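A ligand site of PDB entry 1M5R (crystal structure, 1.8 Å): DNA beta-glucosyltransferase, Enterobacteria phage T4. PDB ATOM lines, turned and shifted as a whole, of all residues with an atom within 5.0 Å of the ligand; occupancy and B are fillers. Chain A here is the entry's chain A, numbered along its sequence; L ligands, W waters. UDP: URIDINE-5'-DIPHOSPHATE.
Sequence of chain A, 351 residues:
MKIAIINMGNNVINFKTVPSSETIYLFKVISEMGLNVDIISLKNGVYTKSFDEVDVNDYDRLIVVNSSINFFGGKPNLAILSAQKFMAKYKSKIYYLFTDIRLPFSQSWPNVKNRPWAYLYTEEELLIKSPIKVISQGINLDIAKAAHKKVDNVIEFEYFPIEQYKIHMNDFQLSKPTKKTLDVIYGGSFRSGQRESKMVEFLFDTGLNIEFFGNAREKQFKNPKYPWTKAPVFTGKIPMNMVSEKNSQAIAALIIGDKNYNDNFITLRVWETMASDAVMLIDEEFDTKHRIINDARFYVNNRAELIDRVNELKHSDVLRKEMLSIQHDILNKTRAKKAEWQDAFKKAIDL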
ATOM      1  N   VAL A  18     -24.287   4.176 -32.750  1.00  0.00           N
ATOM      2  CA  VAL A  18     -25.004   3.164 -33.513  1.00  0.00           C
ATOM      3  C   VAL A  18     -25.521   3.678 -34.855  1.00  0.00           C
ATOM      4  O   VAL A  18     -25.421   2.985 -35.861  1.00  0.00           O
ATOM      5  CB  VAL A  18     -26.146   2.549 -32.667  1.00  0.00           C
ATOM      6  CG1 VAL A  18     -26.919   1.532 -33.488  1.00  0.00           C
ATOM      7  CG2 VAL A  18     -25.548   1.888 -31.423  1.00  0.00           C
ATOM      8  N   ASP A 100     -35.971   0.745 -37.924  1.00  0.00           N
ATOM      9  CA  ASP A 100     -36.450   0.910 -36.549  1.00  0.00           C
ATOM     10  C   ASP A 100     -37.890   1.432 -36.574  1.00  0.00           C
ATOM     11  O   ASP A 100     -38.152   2.509 -37.115  1.00  0.00           O
ATOM     12  CB  ASP A 100     -35.521   1.886 -35.821  1.00  0.00           C
ATOM     13  CG  ASP A 100     -35.791   1.963 -34.331  1.00  0.00           C
ATOM     14  OD1 ASP A 100     -34.816   2.133 -33.559  1.00  0.00           O
ATOM     15  OD2 ASP A 100     -36.974   1.884 -33.916  1.00  0.00           O
ATOM     16  N   TYR A 186     -26.843  -8.315 -22.552  1.00  0.00           N
ATOM     17  CA  TYR A 186     -27.729  -7.652 -23.493  1.00  0.00           C
ATOM     18  C   TYR A 186     -27.189  -6.254 -23.740  1.00  0.00           C
ATOM     19  O   TYR A 186     -26.857  -5.534 -22.801  1.00  0.00           O
ATOM     20  CB  TYR A 186     -29.161  -7.579 -22.935  1.00  0.00           C
ATOM     21  CG  TYR A 186     -30.127  -6.769 -23.778  1.00  0.00           C
ATOM     22  CD1 TYR A 186     -30.167  -5.375 -23.694  1.00  0.00           C
ATOM     23  CD2 TYR A 186     -30.996  -7.389 -24.665  1.00  0.00           C
ATOM     24  CE1 TYR A 186     -31.036  -4.626 -24.468  1.00  0.00           C
ATOM     25  CE2 TYR A 186     -31.882  -6.651 -25.453  1.00  0.00           C
ATOM     26  CZ  TYR A 186     -31.902  -5.269 -25.347  1.00  0.00           C
ATOM     27  OH  TYR A 186     -32.786  -4.536 -26.099  1.00  0.00           O
ATOM     28  N   GLY A 187     -27.065  -5.876 -25.010  1.00  0.00           N
ATOM     29  CA  GLY A 187     -26.565  -4.548 -25.319  1.00  0.00           C
ATOM     30  C   GLY A 187     -27.556  -3.736 -26.134  1.00  0.00           C
ATOM     31  O   GLY A 187     -28.108  -4.220 -27.123  1.00  0.00           O
ATOM     32  N   GLY A 188     -27.803  -2.505 -25.696  1.00  0.00           N
ATOM     33  CA  GLY A 188     -28.718  -1.647 -26.419  1.00  0.00           C
ATOM     34  C   GLY A 188     -29.005  -0.373 -25.658  1.00  0.00           C
ATOM     35  O   GLY A 188     -28.350  -0.091 -24.644  1.00  0.00           O
ATOM     36  N   SER A 189     -29.976   0.403 -26.131  1.00  0.00           N
ATOM     37  CA  SER A 189     -30.354   1.632 -25.457  1.00  0.00           C
ATOM     38  C   SER A 189     -31.669   1.369 -24.742  1.00  0.00           C
ATOM     39  O   SER A 189     -32.197   0.256 -24.781  1.00  0.00           O
ATOM     40  CB  SER A 189     -30.554   2.766 -26.459  1.00  0.00           C
ATOM     41  OG  SER A 189     -31.805   2.637 -27.106  1.00  0.00           O
ATOM     42  N   ARG A 191     -34.409   2.685 -25.582  1.00  0.00           N
ATOM     43  CA  ARG A 191     -35.443   2.722 -26.611  1.00  0.00           C
ATOM     44  C   ARG A 191     -36.712   3.437 -26.150  1.00  0.00           C
ATOM     45  O   ARG A 191     -37.831   3.040 -26.486  1.00  0.00           O
ATOM     46  CB  ARG A 191     -35.790   1.290 -27.080  1.00  0.00           C
ATOM     47  CG  ARG A 191     -34.705   0.608 -27.902  1.00  0.00           C
ATOM     48  CD  ARG A 191     -35.222  -0.666 -28.572  1.00  0.00           C
ATOM     49  NE  ARG A 191     -36.350  -0.387 -29.464  1.00  0.00           N
ATOM     50  CZ  ARG A 191     -36.236   0.232 -30.637  1.00  0.00           C
ATOM     51  NH1 ARG A 191     -35.052   0.646 -31.078  1.00  0.00           N
ATOM     52  NH2 ARG A 191     -37.323   0.463 -31.370  1.00  0.00           N
ATOM     53  N   ARG A 195     -39.579  -1.070 -24.563  1.00  0.00           N
ATOM     54  CA  ARG A 195     -39.330  -2.461 -24.245  1.00  0.00           C
ATOM     55  C   ARG A 195     -39.058  -2.644 -22.744  1.00  0.00           C
ATOM     56  O   ARG A 195     -38.448  -3.635 -22.330  1.00  0.00           O
ATOM     57  CB  ARG A 195     -38.105  -2.896 -25.065  1.00  0.00           C
ATOM     58  CG  ARG A 195     -37.880  -4.359 -25.197  1.00  0.00           C
ATOM     59  CD  ARG A 195     -36.681  -4.582 -26.124  1.00  0.00           C
ATOM     60  NE  ARG A 195     -36.920  -4.077 -27.473  1.00  0.00           N
ATOM     61  CZ  ARG A 195     -36.012  -4.102 -28.458  1.00  0.00           C
ATOM     62  NH1 ARG A 195     -34.802  -4.599 -28.222  1.00  0.00           N
ATOM     63  NH2 ARG A 195     -36.307  -3.641 -29.665  1.00  0.00           N
ATOM     64  N   PHE A 213     -25.082  -3.657 -21.444  1.00  0.00           N
ATOM     65  CA  PHE A 213     -24.197  -2.635 -21.986  1.00  0.00           C
ATOM     66  C   PHE A 213     -24.910  -1.776 -23.020  1.00  0.00           C
ATOM     67  O   PHE A 213     -25.942  -2.179 -23.552  1.00  0.00           O
ATOM     68  CB  PHE A 213     -22.902  -3.240 -22.578  1.00  0.00           C
ATOM     69  CG  PHE A 213     -23.097  -4.082 -23.828  1.00  0.00           C
ATOM     70  CD1 PHE A 213     -23.460  -5.419 -23.741  1.00  0.00           C
ATOM     71  CD2 PHE A 213     -22.829  -3.538 -25.092  1.00  0.00           C
ATOM     72  CE1 PHE A 213     -23.549  -6.223 -24.890  1.00  0.00           C
ATOM     73  CE2 PHE A 213     -22.913  -4.331 -26.249  1.00  0.00           C
ATOM     74  CZ  PHE A 213     -23.270  -5.679 -26.147  1.00  0.00           C
ATOM     75  N   GLY A 214     -24.362  -0.600 -23.280  1.00  0.00           N
ATOM     76  CA  GLY A 214     -24.968   0.297 -24.243  1.00  0.00           C
ATOM     77  C   GLY A 214     -25.292   1.649 -23.621  1.00  0.00           C
ATOM     78  O   GLY A 214     -24.715   2.017 -22.598  1.00  0.00           O
ATOM     79  N   GLY A 236     -21.015   0.980 -20.041  1.00  0.00           N
ATOM     80  CA  GLY A 236     -21.088   1.912 -21.153  1.00  0.00           C
ATOM     81  C   GLY A 236     -21.268   1.331 -22.531  1.00  0.00           C
ATOM     82  O   GLY A 236     -21.290   0.111 -22.722  1.00  0.00           O
ATOM     83  N   LYS A 237     -21.405   2.213 -23.515  1.00  0.00           N
ATOM     84  CA  LYS A 237     -21.587   1.765 -24.885  1.00  0.00           C
ATOM     85  C   LYS A 237     -20.253   1.418 -25.500  1.00  0.00           C
ATOM     86  O   LYS A 237     -19.206   1.948 -25.106  1.00  0.00           O
ATOM     87  CB  LYS A 237     -22.281   2.856 -25.708  1.00  0.00           C
ATOM     88  CG  LYS A 237     -21.435   4.085 -26.004  1.00  0.00           C
ATOM     89  CD  LYS A 237     -22.224   5.065 -26.854  1.00  0.00           C
ATOM     90  CE  LYS A 237     -21.462   6.351 -27.105  1.00  0.00           C
ATOM     91  NZ  LYS A 237     -22.290   7.372 -27.823  1.00  0.00           N
ATOM     92  N   ILE A 238     -20.276   0.507 -26.466  1.00  0.00           N
ATOM     93  CA  ILE A 238     -19.061   0.106 -27.160  1.00  0.00           C
ATOM     94  C   ILE A 238     -19.323   0.236 -28.666  1.00  0.00           C
ATOM     95  O   ILE A 238     -20.460   0.300 -29.097  1.00  0.00           O
ATOM     96  CB  ILE A 238     -18.689  -1.350 -26.857  1.00  0.00           C
ATOM     97  CG1 ILE A 238     -19.803  -2.278 -27.309  1.00  0.00           C
ATOM     98  CG2 ILE A 238     -18.433  -1.527 -25.357  1.00  0.00           C
ATOM     99  CD1 ILE A 238     -19.394  -3.713 -27.373  1.00  0.00           C
ATOM    100  N   PRO A 239     -18.248   0.301 -29.472  1.00  0.00           N
ATOM    101  CA  PRO A 239     -18.394   0.416 -30.925  1.00  0.00           C
ATOM    102  C   PRO A 239     -19.171  -0.765 -31.492  1.00  0.00           C
ATOM    103  O   PRO A 239     -18.994  -1.893 -31.044  1.00  0.00           O
ATOM    104  CB  PRO A 239     -16.950   0.437 -31.415  1.00  0.00           C
ATOM    105  CG  PRO A 239     -16.200   1.056 -30.255  1.00  0.00           C
ATOM    106  CD  PRO A 239     -16.830   0.354 -29.073  1.00  0.00           C
ATOM    107  N   MET A 240     -20.031  -0.516 -32.482  1.00  0.00           N
ATOM    108  CA  MET A 240     -20.823  -1.597 -33.046  1.00  0.00           C
ATOM    109  C   MET A 240     -20.023  -2.787 -33.597  1.00  0.00           C
ATOM    110  O   MET A 240     -20.462  -3.929 -33.498  1.00  0.00           O
ATOM    111  CB  MET A 240     -21.731  -1.066 -34.160  1.00  0.00           C
ATOM    112  CG  MET A 240     -22.609  -2.162 -34.762  1.00  0.00           C
ATOM    113  SD  MET A 240     -23.623  -1.645 -36.133  1.00  0.00           S
ATOM    114  CE  MET A 240     -25.037  -0.968 -35.292  1.00  0.00           C
ATOM    115  N   VAL A 243     -19.563  -5.604 -30.991  1.00  0.00           N
ATOM    116  CA  VAL A 243     -20.707  -6.178 -30.289  1.00  0.00           C
ATOM    117  C   VAL A 243     -20.706  -7.700 -30.128  1.00  0.00           C
ATOM    118  O   VAL A 243     -21.027  -8.195 -29.044  1.00  0.00           O
ATOM    119  CB  VAL A 243     -22.025  -5.713 -30.931  1.00  0.00           C
ATOM    120  CG1 VAL A 243     -23.211  -6.444 -30.316  1.00  0.00           C
ATOM    121  CG2 VAL A 243     -22.189  -4.198 -30.720  1.00  0.00           C
ATOM    122  N   ILE A 256     -34.794  -9.926 -27.345  1.00  0.00           N
ATOM    123  CA  ILE A 256     -36.146  -9.434 -27.097  1.00  0.00           C
ATOM    124  C   ILE A 256     -36.371  -8.298 -28.071  1.00  0.00           C
ATOM    125  O   ILE A 256     -35.419  -7.797 -28.670  1.00  0.00           O
ATOM    126  CB  ILE A 256     -36.342  -8.894 -25.649  1.00  0.00           C
ATOM    127  CG1 ILE A 256     -35.222  -7.918 -25.284  1.00  0.00           C
ATOM    128  CG2 ILE A 256     -36.429 -10.059 -24.669  1.00  0.00           C
ATOM    129  CD1 ILE A 256     -35.427  -7.230 -23.934  1.00  0.00           C
ATOM    130  N   TYR A 261     -42.258  -5.830 -33.162  1.00  0.00           N
ATOM    131  CA  TYR A 261     -41.169  -6.576 -33.791  1.00  0.00           C
ATOM    132  C   TYR A 261     -41.495  -8.067 -33.747  1.00  0.00           C
ATOM    133  O   TYR A 261     -41.019  -8.832 -34.584  1.00  0.00           O
ATOM    134  CB  TYR A 261     -39.835  -6.356 -33.046  1.00  0.00           C
ATOM    135  CG  TYR A 261     -39.156  -5.031 -33.322  1.00  0.00           C
ATOM    136  CD1 TYR A 261     -39.693  -4.112 -34.219  1.00  0.00           C
ATOM    137  CD2 TYR A 261     -37.947  -4.704 -32.690  1.00  0.00           C
ATOM    138  CE1 TYR A 261     -39.057  -2.906 -34.485  1.00  0.00           C
ATOM    139  CE2 TYR A 261     -37.299  -3.498 -32.948  1.00  0.00           C
ATOM    140  CZ  TYR A 261     -37.867  -2.607 -33.852  1.00  0.00           C
ATOM    141  OH  TYR A 261     -37.235  -1.412 -34.111  1.00  0.00           O
ATOM    142  N   THR A 267     -33.822  -8.514 -35.982  1.00  0.00           N
ATOM    143  CA  THR A 267     -32.977  -7.364 -35.687  1.00  0.00           C
ATOM    144  C   THR A 267     -31.498  -7.704 -35.704  1.00  0.00           C
ATOM    145  O   THR A 267     -31.114  -8.875 -35.686  1.00  0.00           O
ATOM    146  CB  THR A 267     -33.329  -6.800 -34.295  1.00  0.00           C
ATOM    147  OG1 THR A 267     -33.223  -7.860 -33.327  1.00  0.00           O
ATOM    148  CG2 THR A 267     -34.765  -6.248 -34.285  1.00  0.00           C
ATOM    149  N   LEU A 268     -30.661  -6.668 -35.738  1.00  0.00           N
ATOM    150  CA  LEU A 268     -29.219  -6.874 -35.753  1.00  0.00           C
ATOM    151  C   LEU A 268     -28.725  -7.818 -34.665  1.00  0.00           C
ATOM    152  O   LEU A 268     -27.859  -8.665 -34.914  1.00  0.00           O
ATOM    153  CB  LEU A 268     -28.488  -5.541 -35.574  1.00  0.00           C
ATOM    154  CG  LEU A 268     -28.234  -4.695 -36.815  1.00  0.00           C
ATOM    155  CD1 LEU A 268     -27.729  -3.325 -36.389  1.00  0.00           C
ATOM    156  CD2 LEU A 268     -27.220  -5.394 -37.723  1.00  0.00           C
ATOM    157  N   ARG A 269     -29.287  -7.688 -33.454  1.00  0.00           N
ATOM    158  CA  ARG A 269     -28.838  -8.525 -32.342  1.00  0.00           C
ATOM    159  C   ARG A 269     -29.052 -10.020 -32.585  1.00  0.00           C
ATOM    160  O   ARG A 269     -28.340 -10.837 -32.005  1.00  0.00           O
ATOM    161  CB  ARG A 269     -29.498  -8.109 -31.024  1.00  0.00           C
ATOM    162  CG  ARG A 269     -30.985  -8.396 -30.922  1.00  0.00           C
ATOM    163  CD  ARG A 269     -31.524  -8.041 -29.520  1.00  0.00           C
ATOM    164  NE  ARG A 269     -31.449  -6.607 -29.257  1.00  0.00           N
ATOM    165  CZ  ARG A 269     -30.473  -6.006 -28.571  1.00  0.00           C
ATOM    166  NH1 ARG A 269     -29.458  -6.720 -28.071  1.00  0.00           N
ATOM    167  NH2 ARG A 269     -30.507  -4.697 -28.407  1.00  0.00           N
ATOM    168  N   GLU A 272     -25.910 -10.748 -34.409  1.00  0.00           N
ATOM    169  CA  GLU A 272     -24.739 -10.476 -33.571  1.00  0.00           C
ATOM    170  C   GLU A 272     -24.615 -11.491 -32.441  1.00  0.00           C
ATOM    171  O   GLU A 272     -23.516 -11.813 -32.001  1.00  0.00           O
ATOM    172  CB  GLU A 272     -24.819  -9.080 -32.964  1.00  0.00           C
ATOM    173  CG  GLU A 272     -24.946  -7.951 -33.978  1.00  0.00           C
ATOM    174  CD  GLU A 272     -25.268  -6.620 -33.306  1.00  0.00           C
ATOM    175  OE1 GLU A 272     -26.051  -6.626 -32.337  1.00  0.00           O
ATOM    176  OE2 GLU A 272     -24.754  -5.576 -33.760  1.00  0.00           O
HETATM  177  N1  UDP L   1     -25.095  -1.471 -29.966  1.00  0.00           N
HETATM  178  C2  UDP L   1     -23.813  -0.972 -30.117  1.00  0.00           C
HETATM  179  N3  UDP L   1     -23.148  -0.725 -28.946  1.00  0.00           N
HETATM  180  C4  UDP L   1     -23.627  -0.916 -27.658  1.00  0.00           C
HETATM  181  C5  UDP L   1     -24.954  -1.455 -27.585  1.00  0.00           C
HETATM  182  C6  UDP L   1     -25.624  -1.712 -28.720  1.00  0.00           C
HETATM  183  O2  UDP L   1     -23.294  -0.771 -31.214  1.00  0.00           O
HETATM  184  O4  UDP L   1     -22.938  -0.555 -26.695  1.00  0.00           O
HETATM  185  C1' UDP L   1     -25.865  -1.738 -31.197  1.00  0.00           C
HETATM  186  C2' UDP L   1     -25.859  -3.206 -31.647  1.00  0.00           C
HETATM  187  O2' UDP L   1     -25.716  -3.250 -33.050  1.00  0.00           O
HETATM  188  C3' UDP L   1     -27.228  -3.683 -31.166  1.00  0.00           C
HETATM  189  C4' UDP L   1     -28.081  -2.458 -31.376  1.00  0.00           C
HETATM  190  O4' UDP L   1     -27.214  -1.363 -30.973  1.00  0.00           O
HETATM  191  O3' UDP L   1     -27.730  -4.753 -31.971  1.00  0.00           O
HETATM  192  C5' UDP L   1     -29.376  -2.437 -30.600  1.00  0.00           C
HETATM  193  O5' UDP L   1     -30.102  -1.245 -30.883  1.00  0.00           O
HETATM  194  PA  UDP L   1     -31.397  -0.869 -30.034  1.00  0.00           P
HETATM  195  O1A UDP L   1     -30.927  -0.483 -28.675  1.00  0.00           O
HETATM  196  O2A UDP L   1     -32.213   0.097 -30.828  1.00  0.00           O
HETATM  197  O3A UDP L   1     -32.183  -2.285 -29.886  1.00  0.00           O
HETATM  198  PB  UDP L   1     -32.919  -3.227 -31.006  1.00  0.00           P
HETATM  199  O1B UDP L   1     -32.007  -3.236 -32.211  1.00  0.00           O
HETATM  200  O2B UDP L   1     -34.255  -2.568 -31.259  1.00  0.00           O
HETATM  201  O3B UDP L   1     -33.036  -4.586 -30.324  1.00  0.00           O
HETATM  202  O   HOH W   1     -21.728   2.043 -32.225  1.00  0.00           O
HETATM  203  O   HOH W   2     -31.883   2.695 -29.934  1.00  0.00           O
HETATM  204  O   HOH W   3     -28.283   0.596 -29.155  1.00  0.00           O
HETATM  205  O   HOH W   4     -34.293  -6.897 -31.020  1.00  0.00           O
HETATM  206  O   HOH W   5     -30.409  -5.355 -32.620  1.00  0.00           O
HETATM  207  O   HOH W   6     -34.664  -1.576 -33.691  1.00  0.00           O
HETATM  208  O   HOH W   7     -32.291  -2.034 -26.592  1.00  0.00           O
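Val 18 touches the ligand.
C of Gly 187 touches C5 of the ligand, 3.8 Å away.
Gly 188 touches the ligand (CA to O1A, 3.4 Å).
CD2 of Phe 213 touches O4 of the ligand, 3.4 Å away.
CA of Gly 214 touches O4 of the ligand (3.3 Å).
Lys 237 touches the ligand (CA to O4, 3.2 Å).
CA of Met 240 touches O2 of the ligand (3.2 Å).
Val 243 touches the ligand.
Tyr 261 touches the ligand.
Leu 268 touches the ligand.
Hydrophobic or aromatic side chains within 4 Å of the ligand: Val 18, Phe 213, Ile 238, Met 240, Val 243, Tyr 261 and Leu 268.
The nearest printed residue that does not touch the ligand is Pro 239 (4.1 Å).
Water W6 lies within hydrogen-bond range of the side-chain hydroxyl (OH) of Tyr 261 (2.6 Å), an oxygen (O2B) of the ligand (2.7 Å) and the guanidinium group (NH1) of Arg 191 (3.5 Å).
Water W5 lies within hydrogen-bond range of O1B of the ligand (2.7 Å), N of Arg 269 (2.7 Å) and N of Leu 268 (3.4 Å).
Water W4 lies within hydrogen-bond range of OG1 of Thr 267 (2.7 Å), O3B of the ligand (2.7 Å), O of Ile 256 (2.8 Å) and NE of Arg 269 (3.4 Å).
Water W3 lies within hydrogen-bond range of O4' of the ligand (2.9 Å) and N of Ser 189 (3.5 Å).
Water W7 lies within hydrogen-bond range of the side-chain hydroxyl (OH) of Tyr 186, the backbone carbonyl oxygen (O) of Ser 189 and an oxygen (O1A) of the ligand.
Water W1 lies within hydrogen-bond range of the backbone NH (N) of Met 240 (3.1 Å), the backbone NH (N) of Val 18 (3.4 Å) and an oxygen (O2) of the ligand (3.4 Å).
The side-chain carboxylate (OE1) of Glu 272 lies within hydrogen-bond range of an oxygen (O3') of the ligand.
An oxygen (O3B) of the ligand lies within salt-bridge range of the guanidinium group of Arg 269.
NH1 of Arg 195 lies within salt-bridge range of O3B of the ligand, 2.7 Å away.
NH1 of Arg 191 lies within salt-bridge range of O2A of the ligand.
O1A of the ligand is in hydrogen-bond range of N of Ser 189.
The backbone NH (N) of Ile 238 is in hydrogen-bond range of an oxygen (O4) of the ligand (2.9 Å).
O of Ile 238 is in hydrogen-bond range of N3 of the ligand (2.9 Å).
The backbone carbonyl oxygen of Gly 214 sits at hydrogen-bond distance from the backbone NH of Lys 237 (3.4 Å).
NH1 of Arg 195 sits at hydrogen-bond distance from O of Ile 256, 3.3 Å away.
The backbone carbonyl oxygen (O) of Phe 213 is in hydrogen-bond range of the backbone NH (N) of Gly 188, 2.9 Å away.
The backbone carbonyl oxygen (O) of Tyr 186 is in hydrogen-bond range of the backbone NH (N) of Phe 213 (2.9 Å).
NH1 of Arg 195 is in hydrogen-bond range of OH of Tyr 186, 2.9 Å away.
The side-chain hydroxyl (OH) of Tyr 261 is in hydrogen-bond range of the side-chain carboxylate (OD2) of Asp 100.
The backbone NH (N) of Gly 214 is in hydrogen-bond range of the backbone carbonyl oxygen (O) of Gly 236 (3.2 Å).
The guanidinium group (NH1) of Arg 191 lies within salt-bridge range of the side-chain carboxylate (OD1) of Asp 100 (2.9 Å).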
